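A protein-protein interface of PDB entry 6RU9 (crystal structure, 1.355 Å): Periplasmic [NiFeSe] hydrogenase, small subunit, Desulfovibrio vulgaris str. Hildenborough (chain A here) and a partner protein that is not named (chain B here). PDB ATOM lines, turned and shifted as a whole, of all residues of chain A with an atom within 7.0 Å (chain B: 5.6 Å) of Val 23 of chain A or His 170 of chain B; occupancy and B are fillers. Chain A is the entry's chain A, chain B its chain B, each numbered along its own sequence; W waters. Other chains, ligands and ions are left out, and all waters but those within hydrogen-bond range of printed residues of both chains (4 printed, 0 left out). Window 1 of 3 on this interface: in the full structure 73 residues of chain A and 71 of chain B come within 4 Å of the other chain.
Among the printed residues, merely in contact across the chains: Asn 253 of chain A with Glu 171 of chain B, Asn 27 of chain A with Arg 167 of chain B, Pro 160 of chain A with Pro 181 of chain B, Asn 253 of chain A with Ala 174 of chain B, Val 23 of chain A with His 170 of chain B, Asn 27 of chain A with Met 180 of chain B, Val 256 of chain A with Ala 174 of chain B, Val 256 of chain A with Leu 175 of chain B, Gly 20 of chain A with Gly 73 of chain B, Val 23 of chain A with Arg 166 of chain B, Val 256 of chain A with Glu 171 of chain B, Val 23 of chain A with Pro 181 of chain B, Leu 26 of chain A with Leu 117 of chain B, Gly 20 of chain A with Pro 181 of chain B, Ser 28 of chain A with Arg 167 of chain B, Asn 253 of chain A with His 170 of chain B, Val 23 of chain A with Val 74 of chain B and Val 23 of chain A with Gly 73 of chain B.
OE2 of Glu 77 of chain A is in hydrogen-bond range of N of Gly 20 of chain A (3.4 Å). The backbone carbonyl oxygen (O) of Val 74 of chain B sits at hydrogen-bond distance from the side-chain amide nitrogen (ND2) of Asn 110 of chain B (2.9 Å). The side-chain amide nitrogen (NE2) of Gln 113 of chain B lies within hydrogen-bond range of a ring nitrogen (NE2) of His 170 of chain B. OD1 of Asn 110 of chain B lies within hydrogen-bond range of NE2 of His 170 of chain B, at 2.9 Å. The side-chain carboxylate (OE2) of Glu 171 of chain B lies within salt-bridge range of the guanidinium group (NH1) of Arg 167 of chain B (2.5 Å). The guanidinium group of Arg 166 of chain B is in hydrogen-bond range of a ring nitrogen (ND1) of His 170 of chain B.
ND1 of His 170 of chain B lies within hydrogen-bond range of ND2 of Asn 27 of chain A (3.1 Å). O of Leu 26 of chain A lies within hydrogen-bond range of NH1 of Arg 166 of chain B (3.5 Å). OD1 of Asn 27 of chain A is in hydrogen-bond range of NH1 of Arg 166 of chain B (2.8 Å). O of Cys 18 of chain A is in hydrogen-bond range of N of Gly 73 of chain B, at 2.8 Å. N of Met 180 of chain B sits at hydrogen-bond distance from OD1 of Asn 253 of chain A (2.9 Å).
Hydrophobic or aromatic side chains of chain A within 4 Å of the printed part of chain B: Val 23, Leu 26, Pro 160 and Val 256. Among the printed residues, 23 pairs touch across the chains.
Water W1 bridges O of Leu 26 of chain A (2.8 Å) and NH1 of Arg 166 of chain B (2.9 Å). Water W4 lies within hydrogen-bond range of OG1 of Thr 24 of chain A (2.8 Å), O of Met 180 of chain B (2.8 Å) and ND2 of Asn 27 of chain A (3.0 Å). Water W3 bridges the backbone carbonyl oxygen (O) of Asn 27 of chain A and the guanidinium group (NH1) of Arg 167 of chain B. Water W2 bridges ND2 of Asn 253 of chain A and O of Arg 167 of chain B.
Of the printed residues of chain B, Cys 18 of chain A touches Gly 73. Of the printed residues of chain B, Val 23 of chain A touches Gly 73 (3.9 Å), Val 74 (3.9 Å), Arg 166 (3.7 Å), His 170 (3.5 Å) and Pro 181 (3.7 Å). Of the printed residues of chain B, Leu 26 of chain A touches Leu 117 and Arg 166. Of the printed residues of chain B, Ser 28 of chain A touches Arg 167. Gln 113 of chain B touches none of the printed residues of chain A. Ile 168 of chain B touches none of the printed residues of chain A. Of the printed residues of chain A, Glu 171 of chain B touches Asn 253 and Val 256. Printed residues of chain A within 4 Å of Leu 175 of chain B: Val 256. The nearest residue of chain A that does not touch His 170 of chain B is Val 256 of chain A (5.5 Å).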
ATOM      1  N   TRP A  12     -10.141  28.476  -8.000  1.00  0.00           N
ATOM      2  CA  TRP A  12     -10.364  28.173  -9.409  1.00  0.00           C
ATOM      3  C   TRP A  12     -11.159  29.326  -9.996  1.00  0.00           C
ATOM      4  O   TRP A  12     -12.356  29.480  -9.714  1.00  0.00           O
ATOM      5  CB  TRP A  12     -11.135  26.851  -9.510  1.00  0.00           C
ATOM      6  CG  TRP A  12     -11.285  26.292 -10.900  1.00  0.00           C
ATOM      7  CD1 TRP A  12     -11.981  26.848 -11.939  1.00  0.00           C
ATOM      8  CD2 TRP A  12     -10.808  25.039 -11.364  1.00  0.00           C
ATOM      9  NE1 TRP A  12     -11.922  26.030 -13.042  1.00  0.00           N
ATOM     10  CE2 TRP A  12     -11.206  24.911 -12.718  1.00  0.00           C
ATOM     11  CE3 TRP A  12     -10.058  24.012 -10.781  1.00  0.00           C
ATOM     12  CZ2 TRP A  12     -10.876  23.799 -13.487  1.00  0.00           C
ATOM     13  CZ3 TRP A  12      -9.749  22.912 -11.533  1.00  0.00           C
ATOM     14  CH2 TRP A  12     -10.148  22.816 -12.880  1.00  0.00           C
ATOM     15  N   CYS A  18     -15.426  27.580 -21.080  1.00  0.00           N
ATOM     16  CA  CYS A  18     -16.697  26.951 -21.352  1.00  0.00           C
ATOM     17  C   CYS A  18     -17.133  26.002 -20.229  1.00  0.00           C
ATOM     18  O   CYS A  18     -18.159  25.336 -20.390  1.00  0.00           O
ATOM     19  CB  CYS A  18     -16.652  26.194 -22.687  1.00  0.00           C
ATOM     20  SG  CYS A  18     -15.806  24.584 -22.617  1.00  0.00           S
ATOM     21  N   THR A  19     -16.371  25.918 -19.130  1.00  0.00           N
ATOM     22  CA  THR A  19     -16.590  25.016 -17.992  1.00  0.00           C
ATOM     23  C   THR A  19     -16.191  23.589 -18.358  1.00  0.00           C
ATOM     24  O   THR A  19     -16.233  22.689 -17.501  1.00  0.00           O
ATOM     25  CB  THR A  19     -17.992  25.178 -17.406  1.00  0.00           C
ATOM     26  OG1 THR A  19     -18.178  26.587 -17.127  1.00  0.00           O
ATOM     27  CG2 THR A  19     -18.167  24.432 -16.126  1.00  0.00           C
ATOM     28  N   GLY A  20     -15.728  23.362 -19.578  1.00  0.00           N
ATOM     29  CA  GLY A  20     -15.260  22.038 -19.957  1.00  0.00           C
ATOM     30  C   GLY A  20     -14.061  21.550 -19.180  1.00  0.00           C
ATOM     31  O   GLY A  20     -13.914  20.336 -18.983  1.00  0.00           O
ATOM     32  N   CYS A  21     -13.204  22.457 -18.717  1.00  0.00           N
ATOM     33  CA  CYS A  21     -12.031  22.062 -17.933  1.00  0.00           C
ATOM     34  C   CYS A  21     -12.439  21.658 -16.519  1.00  0.00           C
ATOM     35  O   CYS A  21     -11.818  20.772 -15.925  1.00  0.00           O
ATOM     36  CB  CYS A  21     -10.958  23.158 -17.998  1.00  0.00           C
ATOM     37  SG  CYS A  21     -10.220  23.378 -19.682  1.00  0.00           S
ATOM     38  N   SER A  22     -13.497  22.270 -15.979  1.00  0.00           N
ATOM     39  CA  SER A  22     -14.093  21.804 -14.732  1.00  0.00           C
ATOM     40  C   SER A  22     -14.771  20.450 -14.914  1.00  0.00           C
ATOM     41  O   SER A  22     -14.603  19.545 -14.091  1.00  0.00           O
ATOM     42  CB  SER A  22     -15.073  22.826 -14.166  1.00  0.00           C
ATOM     43  OG  SER A  22     -14.366  23.962 -13.691  1.00  0.00           O
ATOM     44  N   VAL A  23     -15.550  20.287 -15.995  1.00  0.00           N
ATOM     45  CA  VAL A  23     -16.279  19.034 -16.203  1.00  0.00           C
ATOM     46  C   VAL A  23     -15.311  17.884 -16.424  1.00  0.00           C
ATOM     47  O   VAL A  23     -15.517  16.782 -15.918  1.00  0.00           O
ATOM     48  CB  VAL A  23     -17.310  19.163 -17.351  1.00  0.00           C
ATOM     49  CG1 VAL A  23     -17.953  17.813 -17.671  1.00  0.00           C
ATOM     50  CG2 VAL A  23     -18.329  20.216 -16.958  1.00  0.00           C
ATOM     51  N   THR A  24     -14.251  18.117 -17.190  1.00  0.00           N
ATOM     52  CA  THR A  24     -13.312  17.021 -17.420  1.00  0.00           C
ATOM     53  C   THR A  24     -12.711  16.574 -16.092  1.00  0.00           C
ATOM     54  O   THR A  24     -12.522  15.379 -15.871  1.00  0.00           O
ATOM     55  CB  THR A  24     -12.261  17.411 -18.458  1.00  0.00           C
ATOM     56  OG1 THR A  24     -11.747  16.206 -19.062  1.00  0.00           O
ATOM     57  CG2 THR A  24     -11.129  18.212 -17.840  1.00  0.00           C
ATOM     58  N   LEU A  25     -12.414  17.526 -15.195  1.00  0.00           N
ATOM     59  CA  LEU A  25     -11.877  17.181 -13.878  1.00  0.00           C
ATOM     60  C   LEU A  25     -12.847  16.285 -13.103  1.00  0.00           C
ATOM     61  O   LEU A  25     -12.432  15.298 -12.464  1.00  0.00           O
ATOM     62  CB  LEU A  25     -11.605  18.462 -13.091  1.00  0.00           C
ATOM     63  CG  LEU A  25     -11.084  18.212 -11.669  1.00  0.00           C
ATOM     64  CD1 LEU A  25      -9.808  17.393 -11.682  1.00  0.00           C
ATOM     65  CD2 LEU A  25     -10.874  19.535 -10.963  1.00  0.00           C
ATOM     66  N   LEU A  26     -14.150  16.604 -13.151  1.00  0.00           N
ATOM     67  CA  LEU A  26     -15.150  15.764 -12.503  1.00  0.00           C
ATOM     68  C   LEU A  26     -15.126  14.319 -12.998  1.00  0.00           C
ATOM     69  O   LEU A  26     -15.681  13.439 -12.330  1.00  0.00           O
ATOM     70  CB  LEU A  26     -16.574  16.310 -12.737  1.00  0.00           C
ATOM     71  CG  LEU A  26     -16.830  17.720 -12.212  1.00  0.00           C
ATOM     72  CD1 LEU A  26     -18.278  18.117 -12.530  1.00  0.00           C
ATOM     73  CD2 LEU A  26     -16.609  17.865 -10.723  1.00  0.00           C
ATOM     74  N   ASN A  27     -14.525  14.053 -14.168  1.00  0.00           N
ATOM     75  CA  ASN A  27     -14.459  12.702 -14.724  1.00  0.00           C
ATOM     76  C   ASN A  27     -13.239  11.908 -14.240  1.00  0.00           C
ATOM     77  O   ASN A  27     -13.009  10.795 -14.727  1.00  0.00           O
ATOM     78  CB  ASN A  27     -14.484  12.741 -16.263  1.00  0.00           C
ATOM     79  CG  ASN A  27     -15.840  13.128 -16.819  1.00  0.00           C
ATOM     80  OD1 ASN A  27     -16.869  12.993 -16.153  1.00  0.00           O
ATOM     81  ND2 ASN A  27     -15.853  13.595 -18.058  1.00  0.00           N
ATOM     82  N   SER A  28     -12.456  12.447 -13.315  1.00  0.00           N
ATOM     83  CA  SER A  28     -11.244  11.758 -12.856  1.00  0.00           C
ATOM     84  C   SER A  28     -11.582  10.386 -12.280  1.00  0.00           C
ATOM     85  O   SER A  28     -12.490  10.262 -11.455  1.00  0.00           O
ATOM     86  CB  SER A  28     -10.536  12.589 -11.796  1.00  0.00           C
ATOM     87  OG  SER A  28      -9.299  11.974 -11.451  1.00  0.00           O
ATOM     88  N   HIS A  46     -14.681  28.135  -6.221  1.00  0.00           N
ATOM     89  CA  HIS A  46     -14.933  27.575  -7.545  1.00  0.00           C
ATOM     90  C   HIS A  46     -16.390  27.905  -7.834  1.00  0.00           C
ATOM     91  O   HIS A  46     -17.291  27.360  -7.176  1.00  0.00           O
ATOM     92  CB  HIS A  46     -14.737  26.079  -7.596  1.00  0.00           C
ATOM     93  CG  HIS A  46     -14.773  25.533  -8.991  1.00  0.00           C
ATOM     94  ND1 HIS A  46     -15.825  25.761  -9.853  1.00  0.00           N
ATOM     95  CD2 HIS A  46     -13.867  24.802  -9.688  1.00  0.00           C
ATOM     96  CE1 HIS A  46     -15.567  25.181 -11.016  1.00  0.00           C
ATOM     97  NE2 HIS A  46     -14.387  24.597 -10.939  1.00  0.00           N
ATOM     98  N   THR A  48     -18.614  27.136  -9.990  1.00  0.00           N
ATOM     99  CA  THR A  48     -19.581  26.151 -10.449  1.00  0.00           C
ATOM    100  C   THR A  48     -20.090  25.256  -9.321  1.00  0.00           C
ATOM    101  O   THR A  48     -21.210  24.716  -9.426  1.00  0.00           O
ATOM    102  CB  THR A  48     -18.948  25.292 -11.552  1.00  0.00           C
ATOM    103  OG1 THR A  48     -18.208  26.118 -12.477  1.00  0.00           O
ATOM    104  CG2 THR A  48     -20.025  24.546 -12.329  1.00  0.00           C
ATOM    105  N   GLU A  77      -9.114  28.801 -15.672  1.00  0.00           N
ATOM    106  CA  GLU A  77      -9.808  28.133 -16.785  1.00  0.00           C
ATOM    107  C   GLU A  77     -10.300  29.254 -17.690  1.00  0.00           C
ATOM    108  O   GLU A  77     -10.982  30.164 -17.215  1.00  0.00           O
ATOM    109  CB  GLU A  77     -10.983  27.306 -16.246  1.00  0.00           C
ATOM    110  CG  GLU A  77     -11.974  26.776 -17.286  1.00  0.00           C
ATOM    111  CD  GLU A  77     -13.030  25.811 -16.695  1.00  0.00           C
ATOM    112  OE1 GLU A  77     -13.268  25.813 -15.468  1.00  0.00           O
ATOM    113  OE2 GLU A  77     -13.636  25.009 -17.462  1.00  0.00           O
ATOM    114  N   PRO A 160     -11.079  19.633 -23.969  1.00  0.00           N
ATOM    115  CA  PRO A 160     -10.455  19.896 -22.674  1.00  0.00           C
ATOM    116  C   PRO A 160      -9.248  19.002 -22.445  1.00  0.00           C
ATOM    117  O   PRO A 160      -9.029  18.048 -23.169  1.00  0.00           O
ATOM    118  CB  PRO A 160     -11.546  19.477 -21.690  1.00  0.00           C
ATOM    119  CG  PRO A 160     -12.174  18.282 -22.390  1.00  0.00           C
ATOM    120  CD  PRO A 160     -12.102  18.571 -23.872  1.00  0.00           C
ATOM    121  N   PRO A 163      -8.654  14.516 -17.442  1.00  0.00           N
ATOM    122  CA  PRO A 163      -8.589  14.716 -15.986  1.00  0.00           C
ATOM    123  C   PRO A 163      -7.259  14.293 -15.407  1.00  0.00           C
ATOM    124  O   PRO A 163      -6.769  14.947 -14.466  1.00  0.00           O
ATOM    125  CB  PRO A 163      -9.743  13.845 -15.442  1.00  0.00           C
ATOM    126  CG  PRO A 163     -10.097  12.939 -16.524  1.00  0.00           C
ATOM    127  CD  PRO A 163      -9.792  13.650 -17.805  1.00  0.00           C
ATOM    128  N   ASN A 253     -12.178   8.945 -20.944  1.00  0.00           N
ATOM    129  CA  ASN A 253     -13.414   8.571 -20.280  1.00  0.00           C
ATOM    130  C   ASN A 253     -13.377   7.117 -19.827  1.00  0.00           C
ATOM    131  O   ASN A 253     -14.184   6.283 -20.226  1.00  0.00           O
ATOM    132  CB  ASN A 253     -14.611   8.871 -21.172  1.00  0.00           C
ATOM    133  CG  ASN A 253     -14.688  10.336 -21.538  1.00  0.00           C
ATOM    134  OD1 ASN A 253     -14.236  10.769 -22.605  1.00  0.00           O
ATOM    135  ND2 ASN A 253     -15.228  11.136 -20.614  1.00  0.00           N
ATOM    136  N   VAL A 256     -12.464   4.170 -22.621  1.00  0.00           N
ATOM    137  CA  VAL A 256     -13.444   3.567 -23.512  1.00  0.00           C
ATOM    138  C   VAL A 256     -13.237   3.951 -24.973  1.00  0.00           C
ATOM    139  O   VAL A 256     -13.784   3.287 -25.862  1.00  0.00           O
ATOM    140  CB  VAL A 256     -14.915   3.854 -23.129  1.00  0.00           C
ATOM    141  CG1 VAL A 256     -15.210   3.260 -21.741  1.00  0.00           C
ATOM    142  CG2 VAL A 256     -15.238   5.344 -23.206  1.00  0.00           C
ATOM    143  N   GLY B  73     -18.901  23.378 -22.207  1.00  0.00           N
ATOM    144  CA  GLY B  73     -18.439  22.045 -21.870  1.00  0.00           C
ATOM    145  C   GLY B  73     -19.391  21.200 -21.057  1.00  0.00           C
ATOM    146  O   GLY B  73     -19.102  20.024 -20.792  1.00  0.00           O
ATOM    147  N   VAL B  74     -20.530  21.764 -20.673  1.00  0.00           N
ATOM    148  CA  VAL B  74     -21.599  21.014 -20.017  1.00  0.00           C
ATOM    149  C   VAL B  74     -22.545  20.408 -21.047  1.00  0.00           C
ATOM    150  O   VAL B  74     -22.952  19.249 -20.905  1.00  0.00           O
ATOM    151  CB  VAL B  74     -22.326  21.904 -19.001  1.00  0.00           C
ATOM    152  CG1 VAL B  74     -23.429  21.119 -18.309  1.00  0.00           C
ATOM    153  CG2 VAL B  74     -21.338  22.492 -17.986  1.00  0.00           C
ATOM    154  N   ALA B 109     -27.189  10.233 -23.747  1.00  0.00           N
ATOM    155  CA  ALA B 109     -26.390   9.964 -22.560  1.00  0.00           C
ATOM    156  C   ALA B 109     -25.989  11.246 -21.855  1.00  0.00           C
ATOM    157  O   ALA B 109     -25.859  11.270 -20.633  1.00  0.00           O
ATOM    158  CB  ALA B 109     -25.136   9.162 -22.922  1.00  0.00           C
ATOM    159  N   ASN B 110     -25.815  12.339 -22.598  1.00  0.00           N
ATOM    160  CA  ASN B 110     -25.457  13.596 -21.922  1.00  0.00           C
ATOM    161  C   ASN B 110     -26.664  14.278 -21.281  1.00  0.00           C
ATOM    162  O   ASN B 110     -26.488  15.048 -20.335  1.00  0.00           O
ATOM    163  CB  ASN B 110     -24.698  14.589 -22.770  1.00  0.00           C
ATOM    164  CG  ASN B 110     -23.952  15.585 -21.913  1.00  0.00           C
ATOM    165  OD1 ASN B 110     -23.195  15.171 -21.009  1.00  0.00           O
ATOM    166  ND2 ASN B 110     -24.229  16.883 -22.091  1.00  0.00           N
ATOM    167  N   GLN B 113     -26.386  12.839 -17.966  1.00  0.00           N
ATOM    168  CA  GLN B 113     -25.283  13.456 -17.239  1.00  0.00           C
ATOM    169  C   GLN B 113     -25.665  14.843 -16.755  1.00  0.00           C
ATOM    170  O   GLN B 113     -25.443  15.199 -15.589  1.00  0.00           O
ATOM    171  CB  GLN B 113     -24.037  13.590 -18.127  1.00  0.00           C
ATOM    172  CG  GLN B 113     -22.815  14.138 -17.382  1.00  0.00           C
ATOM    173  CD  GLN B 113     -22.657  15.660 -17.363  1.00  0.00           C
ATOM    174  OE1 GLN B 113     -22.019  16.201 -16.438  1.00  0.00           O
ATOM    175  NE2 GLN B 113     -23.136  16.347 -18.395  1.00  0.00           N
ATOM    176  N   LEU B 117     -25.967  16.056 -12.904  1.00  0.00           N
ATOM    177  CA  LEU B 117     -25.064  17.116 -12.478  1.00  0.00           C
ATOM    178  C   LEU B 117     -25.840  18.289 -11.921  1.00  0.00           C
ATOM    179  O   LEU B 117     -25.500  18.835 -10.857  1.00  0.00           O
ATOM    180  CB  LEU B 117     -24.236  17.585 -13.674  1.00  0.00           C
ATOM    181  CG  LEU B 117     -23.308  18.770 -13.437  1.00  0.00           C
ATOM    182  CD1 LEU B 117     -22.021  18.338 -12.745  1.00  0.00           C
ATOM    183  CD2 LEU B 117     -22.995  19.428 -14.780  1.00  0.00           C
ATOM    184  N   VAL B 165     -21.990   8.423 -10.931  1.00  0.00           N
ATOM    185  CA  VAL B 165     -23.001   8.159 -11.948  1.00  0.00           C
ATOM    186  C   VAL B 165     -22.844   9.112 -13.126  1.00  0.00           C
ATOM    187  O   VAL B 165     -22.884   8.681 -14.284  1.00  0.00           O
ATOM    188  CB  VAL B 165     -24.410   8.197 -11.336  1.00  0.00           C
ATOM    189  CG1 VAL B 165     -25.441   8.001 -12.410  1.00  0.00           C
ATOM    190  CG2 VAL B 165     -24.537   7.140 -10.285  1.00  0.00           C
ATOM    191  N   ARG B 166     -22.636  10.415 -12.868  1.00  0.00           N
ATOM    192  CA  ARG B 166     -22.463  11.350 -13.983  1.00  0.00           C
ATOM    193  C   ARG B 166     -21.193  11.037 -14.778  1.00  0.00           C
ATOM    194  O   ARG B 166     -21.164  11.235 -15.992  1.00  0.00           O
ATOM    195  CB  ARG B 166     -22.528  12.815 -13.533  1.00  0.00           C
ATOM    196  CG  ARG B 166     -21.398  13.261 -12.648  1.00  0.00           C
ATOM    197  CD  ARG B 166     -20.986  14.725 -12.815  1.00  0.00           C
ATOM    198  NE  ARG B 166     -20.659  14.991 -14.220  1.00  0.00           N
ATOM    199  CZ  ARG B 166     -19.546  14.543 -14.818  1.00  0.00           C
ATOM    200  NH1 ARG B 166     -18.634  13.864 -14.136  1.00  0.00           N
ATOM    201  NH2 ARG B 166     -19.365  14.749 -16.113  1.00  0.00           N
ATOM    202  N   ARG B 167     -20.142  10.520 -14.121  1.00  0.00           N
ATOM    203  CA  ARG B 167     -18.933  10.148 -14.853  1.00  0.00           C
ATOM    204  C   ARG B 167     -19.208   8.963 -15.758  1.00  0.00           C
ATOM    205  O   ARG B 167     -18.719   8.907 -16.895  1.00  0.00           O
ATOM    206  CB  ARG B 167     -17.824   9.830 -13.850  1.00  0.00           C
ATOM    207  CG  ARG B 167     -16.482   9.442 -14.487  1.00  0.00           C
ATOM    208  CD  ARG B 167     -15.460   8.883 -13.455  1.00  0.00           C
ATOM    209  NE  ARG B 167     -15.871   7.534 -13.079  1.00  0.00           N
ATOM    210  CZ  ARG B 167     -15.795   6.498 -13.926  1.00  0.00           C
ATOM    211  NH1 ARG B 167     -15.268   6.679 -15.134  1.00  0.00           N
ATOM    212  NH2 ARG B 167     -16.223   5.302 -13.573  1.00  0.00           N
ATOM    213  N   ILE B 168     -20.017   8.013 -15.284  1.00  0.00           N
ATOM    214  CA  ILE B 168     -20.398   6.868 -16.109  1.00  0.00           C
ATOM    215  C   ILE B 168     -21.210   7.325 -17.311  1.00  0.00           C
ATOM    216  O   ILE B 168     -21.076   6.771 -18.405  1.00  0.00           O
ATOM    217  CB  ILE B 168     -21.144   5.831 -15.249  1.00  0.00           C
ATOM    218  CG1 ILE B 168     -20.178   5.198 -14.243  1.00  0.00           C
ATOM    219  CG2 ILE B 168     -21.808   4.782 -16.100  1.00  0.00           C
ATOM    220  CD1 ILE B 168     -20.886   4.475 -13.101  1.00  0.00           C
ATOM    221  N   CYS B 169     -22.062   8.342 -17.137  1.00  0.00           N
ATOM    222  CA  CYS B 169     -22.800   8.887 -18.276  1.00  0.00           C
ATOM    223  C   CYS B 169     -21.837   9.392 -19.347  1.00  0.00           C
ATOM    224  O   CYS B 169     -22.062   9.196 -20.543  1.00  0.00           O
ATOM    225  CB  CYS B 169     -23.725  10.027 -17.850  1.00  0.00           C
ATOM    226  SG  CYS B 169     -25.133   9.530 -16.820  1.00  0.00           S
ATOM    227  N   HIS B 170     -20.751  10.053 -18.935  1.00  0.00           N
ATOM    228  CA  HIS B 170     -19.769  10.508 -19.925  1.00  0.00           C
ATOM    229  C   HIS B 170     -19.016   9.348 -20.569  1.00  0.00           C
ATOM    230  O   HIS B 170     -18.640   9.442 -21.744  1.00  0.00           O
ATOM    231  CB  HIS B 170     -18.844  11.552 -19.337  1.00  0.00           C
ATOM    232  CG  HIS B 170     -19.382  12.939 -19.498  1.00  0.00           C
ATOM    233  ND1 HIS B 170     -18.656  14.062 -19.182  1.00  0.00           N
ATOM    234  CD2 HIS B 170     -20.578  13.378 -19.952  1.00  0.00           C
ATOM    235  CE1 HIS B 170     -19.383  15.137 -19.421  1.00  0.00           C
ATOM    236  NE2 HIS B 170     -20.558  14.745 -19.883  1.00  0.00           N
ATOM    237  N   GLU B 171     -18.807   8.235 -19.853  1.00  0.00           N
ATOM    238  CA  GLU B 171     -18.294   7.029 -20.519  1.00  0.00           C
ATOM    239  C   GLU B 171     -19.260   6.582 -21.622  1.00  0.00           C
ATOM    240  O   GLU B 171     -18.844   6.169 -22.710  1.00  0.00           O
ATOM    241  CB  GLU B 171     -18.089   5.915 -19.503  1.00  0.00           C
ATOM    242  CG  GLU B 171     -16.971   6.215 -18.494  1.00  0.00           C
ATOM    243  CD  GLU B 171     -16.557   5.026 -17.645  1.00  0.00           C
ATOM    244  OE1 GLU B 171     -17.279   4.007 -17.615  1.00  0.00           O
ATOM    245  OE2 GLU B 171     -15.481   5.114 -17.024  1.00  0.00           O
ATOM    246  N   MET B 172     -20.563   6.615 -21.340  1.00  0.00           N
ATOM    247  CA  MET B 172     -21.568   6.284 -22.352  1.00  0.00           C
ATOM    248  C   MET B 172     -21.444   7.199 -23.563  1.00  0.00           C
ATOM    249  O   MET B 172     -21.457   6.726 -24.710  1.00  0.00           O
ATOM    250  CB  MET B 172     -22.969   6.337 -21.756  1.00  0.00           C
ATOM    251  CG  MET B 172     -23.204   5.238 -20.744  1.00  0.00           C
ATOM    252  SD  MET B 172     -24.667   5.555 -19.731  1.00  0.00           S
ATOM    253  CE  MET B 172     -25.917   5.783 -20.986  1.00  0.00           C
ATOM    254  N   VAL B 173     -21.354   8.511 -23.335  1.00  0.00           N
ATOM    255  CA  VAL B 173     -21.172   9.456 -24.439  1.00  0.00           C
ATOM    256  C   VAL B 173     -19.959   9.076 -25.276  1.00  0.00           C
ATOM    257  O   VAL B 173     -20.006   9.065 -26.515  1.00  0.00           O
ATOM    258  CB  VAL B 173     -21.043  10.906 -23.922  1.00  0.00           C
ATOM    259  CG1 VAL B 173     -20.725  11.851 -25.093  1.00  0.00           C
ATOM    260  CG2 VAL B 173     -22.303  11.335 -23.200  1.00  0.00           C
ATOM    261  N   ALA B 174     -18.829   8.806 -24.605  1.00  0.00           N
ATOM    262  CA  ALA B 174     -17.559   8.580 -25.294  1.00  0.00           C
ATOM    263  C   ALA B 174     -17.503   7.261 -26.048  1.00  0.00           C
ATOM    264  O   ALA B 174     -16.713   7.138 -26.993  1.00  0.00           O
ATOM    265  CB  ALA B 174     -16.403   8.651 -24.291  1.00  0.00           C
ATOM    266  N   LEU B 175     -18.314   6.265 -25.669  1.00  0.00           N
ATOM    267  CA  LEU B 175     -18.269   4.976 -26.361  1.00  0.00           C
ATOM    268  C   LEU B 175     -18.399   5.139 -27.877  1.00  0.00           C
ATOM    269  O   LEU B 175     -17.629   4.545 -28.640  1.00  0.00           O
ATOM    270  CB  LEU B 175     -19.303   4.018 -25.796  1.00  0.00           C
ATOM    271  CG  LEU B 175     -18.816   3.312 -24.531  1.00  0.00           C
ATOM    272  CD1 LEU B 175     -20.027   2.678 -23.798  1.00  0.00           C
ATOM    273  CD2 LEU B 175     -17.781   2.259 -24.826  1.00  0.00           C
ATOM    274  N   MET B 180     -15.458  12.990 -24.004  1.00  0.00           N
ATOM    275  CA  MET B 180     -16.407  13.975 -23.517  1.00  0.00           C
ATOM    276  C   MET B 180     -15.774  14.636 -22.311  1.00  0.00           C
ATOM    277  O   MET B 180     -15.200  13.928 -21.484  1.00  0.00           O
ATOM    278  CB  MET B 180     -17.707  13.256 -23.141  1.00  0.00           C
ATOM    279  CG  MET B 180     -18.840  14.173 -22.801  1.00  0.00           C
ATOM    280  SD  MET B 180     -19.433  15.182 -24.172  1.00  0.00           S
ATOM    281  CE  MET B 180     -20.954  15.729 -23.390  1.00  0.00           C
ATOM    282  N   PRO B 181     -15.868  15.974 -22.159  1.00  0.00           N
ATOM    283  CA  PRO B 181     -16.474  16.936 -23.088  1.00  0.00           C
ATOM    284  C   PRO B 181     -15.857  16.981 -24.480  1.00  0.00           C
ATOM    285  O   PRO B 181     -14.714  16.556 -24.690  1.00  0.00           O
ATOM    286  CB  PRO B 181     -16.264  18.286 -22.390  1.00  0.00           C
ATOM    287  CG  PRO B 181     -16.126  17.964 -20.936  1.00  0.00           C
ATOM    288  CD  PRO B 181     -15.407  16.627 -20.915  1.00  0.00           C
HETATM  289  O   HOH W   1     -18.247  13.465 -11.318  1.00  0.00           O
HETATM  290  O   HOH W   2     -16.059   9.798 -18.073  1.00  0.00           O
HETATM  291  O   HOH W   3     -14.026   8.895 -16.610  1.00  0.00           O
HETATM  292  O   HOH W   4     -13.186  13.853 -19.499  1.00  0.00           O
